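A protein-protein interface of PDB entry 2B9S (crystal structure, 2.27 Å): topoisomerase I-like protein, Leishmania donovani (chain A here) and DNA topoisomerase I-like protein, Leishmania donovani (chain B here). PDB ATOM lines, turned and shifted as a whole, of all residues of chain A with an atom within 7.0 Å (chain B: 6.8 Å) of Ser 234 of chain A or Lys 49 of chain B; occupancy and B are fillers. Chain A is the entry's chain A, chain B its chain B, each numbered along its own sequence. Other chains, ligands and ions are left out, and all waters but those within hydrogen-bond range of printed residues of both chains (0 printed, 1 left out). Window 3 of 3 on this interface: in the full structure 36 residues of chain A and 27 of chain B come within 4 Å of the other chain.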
ATOM      1  N   TRP A   6     -19.670 -13.208  28.379  1.00  0.00           N
ATOM      2  CA  TRP A   6     -20.355 -13.497  29.633  1.00  0.00           C
ATOM      3  C   TRP A   6     -20.819 -14.948  29.687  1.00  0.00           C
ATOM      4  O   TRP A   6     -21.178 -15.457  30.749  1.00  0.00           O
ATOM      5  CB  TRP A   6     -21.546 -12.557  29.822  1.00  0.00           C
ATOM      6  CG  TRP A   6     -22.632 -12.754  28.809  1.00  0.00           C
ATOM      7  CD1 TRP A   6     -22.876 -11.986  27.706  1.00  0.00           C
ATOM      8  CD2 TRP A   6     -23.625 -13.786  28.804  1.00  0.00           C
ATOM      9  NE1 TRP A   6     -23.957 -12.478  27.015  1.00  0.00           N
ATOM     10  CE2 TRP A   6     -24.436 -13.584  27.669  1.00  0.00           C
ATOM     11  CE3 TRP A   6     -23.913 -14.866  29.645  1.00  0.00           C
ATOM     12  CZ2 TRP A   6     -25.509 -14.416  27.357  1.00  0.00           C
ATOM     13  CZ3 TRP A   6     -24.978 -15.690  29.333  1.00  0.00           C
ATOM     14  CH2 TRP A   6     -25.763 -15.461  28.200  1.00  0.00           C
ATOM     15  N   GLU A 150     -23.799  -1.062  24.822  1.00  0.00           N
ATOM     16  CA  GLU A 150     -24.904  -1.876  24.310  1.00  0.00           C
ATOM     17  C   GLU A 150     -25.781  -1.045  23.379  1.00  0.00           C
ATOM     18  O   GLU A 150     -25.960   0.153  23.585  1.00  0.00           O
ATOM     19  CB  GLU A 150     -25.751  -2.461  25.451  1.00  0.00           C
ATOM     20  CG  GLU A 150     -24.967  -3.153  26.572  1.00  0.00           C
ATOM     21  CD  GLU A 150     -24.598  -4.617  26.287  1.00  0.00           C
ATOM     22  OE1 GLU A 150     -24.725  -5.096  25.139  1.00  0.00           O
ATOM     23  OE2 GLU A 150     -24.151  -5.294  27.237  1.00  0.00           O
ATOM     24  N   GLN A 151     -26.305  -1.681  22.339  1.00  0.00           N
ATOM     25  CA  GLN A 151     -27.291  -1.031  21.483  1.00  0.00           C
ATOM     26  C   GLN A 151     -28.619  -0.860  22.242  1.00  0.00           C
ATOM     27  O   GLN A 151     -29.007  -1.719  23.023  1.00  0.00           O
ATOM     28  CB  GLN A 151     -27.511  -1.832  20.201  1.00  0.00           C
ATOM     29  CG  GLN A 151     -26.987  -1.147  18.973  1.00  0.00           C
ATOM     30  CD  GLN A 151     -26.830  -2.082  17.778  1.00  0.00           C
ATOM     31  OE1 GLN A 151     -27.062  -3.287  17.877  1.00  0.00           O
ATOM     32  NE2 GLN A 151     -26.425  -1.521  16.643  1.00  0.00           N
ATOM     33  N   LEU A 231     -33.072  -2.241  25.810  1.00  0.00           N
ATOM     34  CA  LEU A 231     -31.878  -2.623  25.016  1.00  0.00           C
ATOM     35  C   LEU A 231     -32.208  -3.537  23.842  1.00  0.00           C
ATOM     36  O   LEU A 231     -33.259  -4.153  23.820  1.00  0.00           O
ATOM     37  CB  LEU A 231     -30.764  -3.226  25.898  1.00  0.00           C
ATOM     38  CG  LEU A 231     -30.177  -2.388  27.048  1.00  0.00           C
ATOM     39  CD1 LEU A 231     -28.837  -2.934  27.491  1.00  0.00           C
ATOM     40  CD2 LEU A 231     -30.027  -0.934  26.691  1.00  0.00           C
ATOM     41  N   ALA A 232     -31.319  -3.569  22.852  1.00  0.00           N
ATOM     42  CA  ALA A 232     -31.457  -4.430  21.687  1.00  0.00           C
ATOM     43  C   ALA A 232     -31.241  -5.890  22.086  1.00  0.00           C
ATOM     44  O   ALA A 232     -30.597  -6.161  23.091  1.00  0.00           O
ATOM     45  CB  ALA A 232     -30.467  -4.012  20.604  1.00  0.00           C
ATOM     46  N   PRO A 233     -31.798  -6.838  21.310  1.00  0.00           N
ATOM     47  CA  PRO A 233     -31.644  -8.267  21.643  1.00  0.00           C
ATOM     48  C   PRO A 233     -30.181  -8.749  21.659  1.00  0.00           C
ATOM     49  O   PRO A 233     -29.875  -9.732  22.345  1.00  0.00           O
ATOM     50  CB  PRO A 233     -32.459  -8.989  20.558  1.00  0.00           C
ATOM     51  CG  PRO A 233     -33.294  -7.931  19.887  1.00  0.00           C
ATOM     52  CD  PRO A 233     -32.613  -6.618  20.100  1.00  0.00           C
ATOM     53  N   SER A 234     -29.300  -8.041  20.931  1.00  0.00           N
ATOM     54  CA  SER A 234     -27.835  -8.278  20.947  1.00  0.00           C
ATOM     55  C   SER A 234     -27.146  -7.931  22.268  1.00  0.00           C
ATOM     56  O   SER A 234     -25.992  -8.320  22.498  1.00  0.00           O
ATOM     57  CB  SER A 234     -27.130  -7.554  19.782  1.00  0.00           C
ATOM     58  OG  SER A 234     -27.198  -6.136  19.895  1.00  0.00           O
ATOM     59  N   SER A 235     -27.839  -7.205  23.141  1.00  0.00           N
ATOM     60  CA  SER A 235     -27.280  -6.842  24.450  1.00  0.00           C
ATOM     61  C   SER A 235     -27.167  -8.040  25.395  1.00  0.00           C
ATOM     62  O   SER A 235     -27.881  -9.032  25.254  1.00  0.00           O
ATOM     63  CB  SER A 235     -28.089  -5.701  25.101  1.00  0.00           C
ATOM     64  OG  SER A 235     -29.343  -6.162  25.578  1.00  0.00           O
ATOM     65  N   SER A 236     -26.280  -7.944  26.373  1.00  0.00           N
ATOM     66  CA  SER A 236     -26.050  -9.059  27.279  1.00  0.00           C
ATOM     67  C   SER A 236     -27.189  -9.276  28.259  1.00  0.00           C
ATOM     68  O   SER A 236     -27.441 -10.409  28.669  1.00  0.00           O
ATOM     69  CB  SER A 236     -24.708  -8.908  28.015  1.00  0.00           C
ATOM     70  OG  SER A 236     -24.585  -7.635  28.597  1.00  0.00           O
ATOM     71  N   VAL A 237     -27.876  -8.203  28.639  1.00  0.00           N
ATOM     72  CA  VAL A 237     -29.023  -8.323  29.547  1.00  0.00           C
ATOM     73  C   VAL A 237     -30.168  -9.098  28.876  1.00  0.00           C
ATOM     74  O   VAL A 237     -30.899  -9.822  29.546  1.00  0.00           O
ATOM     75  CB  VAL A 237     -29.505  -6.943  30.135  1.00  0.00           C
ATOM     76  CG1 VAL A 237     -30.131  -6.051  29.070  1.00  0.00           C
ATOM     77  CG2 VAL A 237     -30.504  -7.172  31.288  1.00  0.00           C
ATOM     78  N   LYS A 238     -30.296  -8.965  27.553  1.00  0.00           N
ATOM     79  CA  LYS A 238     -31.344  -9.660  26.815  1.00  0.00           C
ATOM     80  C   LYS A 238     -30.914 -11.095  26.602  1.00  0.00           C
ATOM     81  O   LYS A 238     -31.729 -12.006  26.721  1.00  0.00           O
ATOM     82  CB  LYS A 238     -31.631  -9.002  25.459  1.00  0.00           C
ATOM     83  CG  LYS A 238     -32.332  -7.637  25.529  1.00  0.00           C
ATOM     84  CD  LYS A 238     -33.800  -7.725  25.981  1.00  0.00           C
ATOM     85  CE  LYS A 238     -34.438  -6.351  25.944  1.00  0.00           C
ATOM     86  NZ  LYS A 238     -35.826  -6.318  26.491  1.00  0.00           N
ATOM     87  N   GLY A 239     -29.624 -11.274  26.301  1.00  0.00           N
ATOM     88  CA  GLY A 239     -29.044 -12.574  25.988  1.00  0.00           C
ATOM     89  C   GLY A 239     -29.124 -13.497  27.165  1.00  0.00           C
ATOM     90  O   GLY A 239     -29.497 -14.655  27.021  1.00  0.00           O
ATOM     91  N   SER B  44     -30.223 -14.849   9.867  1.00  0.00           N
ATOM     92  CA  SER B  44     -29.700 -13.634   9.260  1.00  0.00           C
ATOM     93  C   SER B  44     -28.608 -13.039  10.151  1.00  0.00           C
ATOM     94  O   SER B  44     -28.401 -13.495  11.275  1.00  0.00           O
ATOM     95  CB  SER B  44     -30.821 -12.619   9.045  1.00  0.00           C
ATOM     96  OG  SER B  44     -31.210 -12.020  10.275  1.00  0.00           O
ATOM     97  N   ALA B  45     -27.906 -12.032   9.633  1.00  0.00           N
ATOM     98  CA  ALA B  45     -26.891 -11.279  10.378  1.00  0.00           C
ATOM     99  C   ALA B  45     -27.373 -10.794  11.752  1.00  0.00           C
ATOM    100  O   ALA B  45     -26.664 -10.917  12.744  1.00  0.00           O
ATOM    101  CB  ALA B  45     -26.447 -10.090   9.555  1.00  0.00           C
ATOM    102  N   THR B  46     -28.573 -10.224  11.782  1.00  0.00           N
ATOM    103  CA  THR B  46     -29.164  -9.652  12.991  1.00  0.00           C
ATOM    104  C   THR B  46     -29.528 -10.715  14.038  1.00  0.00           C
ATOM    105  O   THR B  46     -29.273 -10.515  15.218  1.00  0.00           O
ATOM    106  CB  THR B  46     -30.366  -8.737  12.636  1.00  0.00           C
ATOM    107  OG1 THR B  46     -29.867  -7.471  12.192  1.00  0.00           O
ATOM    108  CG2 THR B  46     -31.256  -8.499  13.818  1.00  0.00           C
ATOM    109  N   ILE B  47     -30.068 -11.849  13.611  1.00  0.00           N
ATOM    110  CA  ILE B  47     -30.417 -12.906  14.562  1.00  0.00           C
ATOM    111  C   ILE B  47     -29.207 -13.730  15.046  1.00  0.00           C
ATOM    112  O   ILE B  47     -29.246 -14.339  16.119  1.00  0.00           O
ATOM    113  CB  ILE B  47     -31.684 -13.746  14.122  1.00  0.00           C
ATOM    114  CG1 ILE B  47     -31.691 -15.149  14.731  1.00  0.00           C
ATOM    115  CG2 ILE B  47     -31.808 -13.838  12.630  1.00  0.00           C
ATOM    116  CD1 ILE B  47     -33.084 -15.686  14.908  1.00  0.00           C
ATOM    117  N   GLN B  48     -28.119 -13.701  14.276  1.00  0.00           N
ATOM    118  CA  GLN B  48     -26.838 -14.218  14.752  1.00  0.00           C
ATOM    119  C   GLN B  48     -26.271 -13.364  15.888  1.00  0.00           C
ATOM    120  O   GLN B  48     -25.762 -13.902  16.872  1.00  0.00           O
ATOM    121  CB  GLN B  48     -25.830 -14.329  13.611  1.00  0.00           C
ATOM    122  CG  GLN B  48     -26.006 -15.581  12.750  1.00  0.00           C
ATOM    123  CD  GLN B  48     -25.060 -15.607  11.568  1.00  0.00           C
ATOM    124  OE1 GLN B  48     -25.491 -15.507  10.412  1.00  0.00           O
ATOM    125  NE2 GLN B  48     -23.760 -15.722  11.847  1.00  0.00           N
ATOM    126  N   LYS B  49     -26.366 -12.040  15.749  1.00  0.00           N
ATOM    127  CA  LYS B  49     -25.940 -11.103  16.798  1.00  0.00           C
ATOM    128  C   LYS B  49     -26.836 -11.167  18.063  1.00  0.00           C
ATOM    129  O   LYS B  49     -26.451 -10.693  19.136  1.00  0.00           O
ATOM    130  CB  LYS B  49     -25.848  -9.650  16.224  1.00  0.00           C
ATOM    131  N   LYS B  50     -28.021 -11.766  17.929  1.00  0.00           N
ATOM    132  CA  LYS B  50     -28.932 -12.013  19.056  1.00  0.00           C
ATOM    133  C   LYS B  50     -28.503 -13.223  19.889  1.00  0.00           C
ATOM    134  O   LYS B  50     -28.719 -13.270  21.111  1.00  0.00           O
ATOM    135  CB  LYS B  50     -30.357 -12.241  18.551  1.00  0.00           C
ATOM    136  CG  LYS B  50     -31.340 -12.552  19.649  1.00  0.00           C
ATOM    137  CD  LYS B  50     -32.741 -12.752  19.159  1.00  0.00           C
ATOM    138  CE  LYS B  50     -33.689 -12.581  20.322  1.00  0.00           C
ATOM    139  NZ  LYS B  50     -35.096 -12.916  19.986  1.00  0.00           N
ATOM    140  N   PHE B  51     -27.886 -14.192  19.221  1.00  0.00           N
ATOM    141  CA  PHE B  51     -27.628 -15.499  19.797  1.00  0.00           C
ATOM    142  C   PHE B  51     -26.133 -15.892  19.903  1.00  0.00           C
ATOM    143  O   PHE B  51     -25.806 -17.072  19.695  1.00  0.00           O
ATOM    144  CB  PHE B  51     -28.353 -16.549  18.956  1.00  0.00           C
ATOM    145  CG  PHE B  51     -29.879 -16.523  19.074  1.00  0.00           C
ATOM    146  CD1 PHE B  51     -30.515 -16.412  20.317  1.00  0.00           C
ATOM    147  CD2 PHE B  51     -30.671 -16.659  17.944  1.00  0.00           C
ATOM    148  CE1 PHE B  51     -31.898 -16.427  20.413  1.00  0.00           C
ATOM    149  CE2 PHE B  51     -32.050 -16.671  18.038  1.00  0.00           C
ATOM    150  CZ  PHE B  51     -32.667 -16.563  19.274  1.00  0.00           C
ATOM    151  N   PRO B  52     -25.230 -14.945  20.280  1.00  0.00           N
ATOM    152  CA  PRO B  52     -23.788 -15.239  20.217  1.00  0.00           C
ATOM    153  C   PRO B  52     -23.343 -16.292  21.231  1.00  0.00           C
ATOM    154  O   PRO B  52     -22.317 -16.942  21.043  1.00  0.00           O
ATOM    155  CB  PRO B  52     -23.154 -13.893  20.570  1.00  0.00           C
ATOM    156  CG  PRO B  52     -24.136 -13.249  21.427  1.00  0.00           C
ATOM    157  CD  PRO B  52     -25.456 -13.595  20.826  1.00  0.00           C
ATOM    158  N   MET B  55     -23.715 -19.815  19.465  1.00  0.00           N
ATOM    159  CA  MET B  55     -23.145 -20.000  18.136  1.00  0.00           C
ATOM    160  C   MET B  55     -22.216 -21.209  18.098  1.00  0.00           C
ATOM    161  O   MET B  55     -21.978 -21.790  17.039  1.00  0.00           O
ATOM    162  CB  MET B  55     -22.391 -18.744  17.696  1.00  0.00           C
ATOM    163  CG  MET B  55     -23.291 -17.561  17.375  1.00  0.00           C
ATOM    164  SD  MET B  55     -24.754 -18.035  16.435  1.00  0.00           S
ATOM    165  CE  MET B  55     -24.026 -18.413  14.843  1.00  0.00           C
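OE1 of Gln 151 of chain A sits at hydrogen-bond distance from OG of Ser 234 of chain A (3.5 Å).
CE of Lys 50 of chain B touches CB of Pro 233 of chain A (3.8 Å).
Ser 234 of chain A touches Lys 49 of chain B (CB to O, 3.3 Å).
Printed residues of chain B that touch a printed residue of chain A: Lys 49 and Lys 50.
Hydrophobic or aromatic side chains of chain A that line the printed part of chain B: Pro 233.
Along chain A the printed residues that touch a printed residue of chain B span positions 233 to 234.
Among the printed residues, 2 pairs touch across the chains.
Among the printed residues, no Asp or Glu carboxylate lies within 4 Å of a Lys or Arg side-chain nitrogen of the other chain.
Of the printed residues of chain B, Ser 234 of chain A touches Lys 49 (3.3 Å).
Lys 49 of chain B touches just one residue of chain A: Ser 234 (3.3 Å).
Printed residues of chain B within 4 Å of Pro 233 of chain A: Lys 50 (3.8 Å).
Printed residues of chain A within 4 Å of Lys 50 of chain B: Pro 233 (3.8 Å).
Trp 6 of chain A touches none of the printed residues of chain B.
The nearest residue of chain B that does not touch Ser 234 of chain A is Lys 50 of chain B (4.3 Å).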
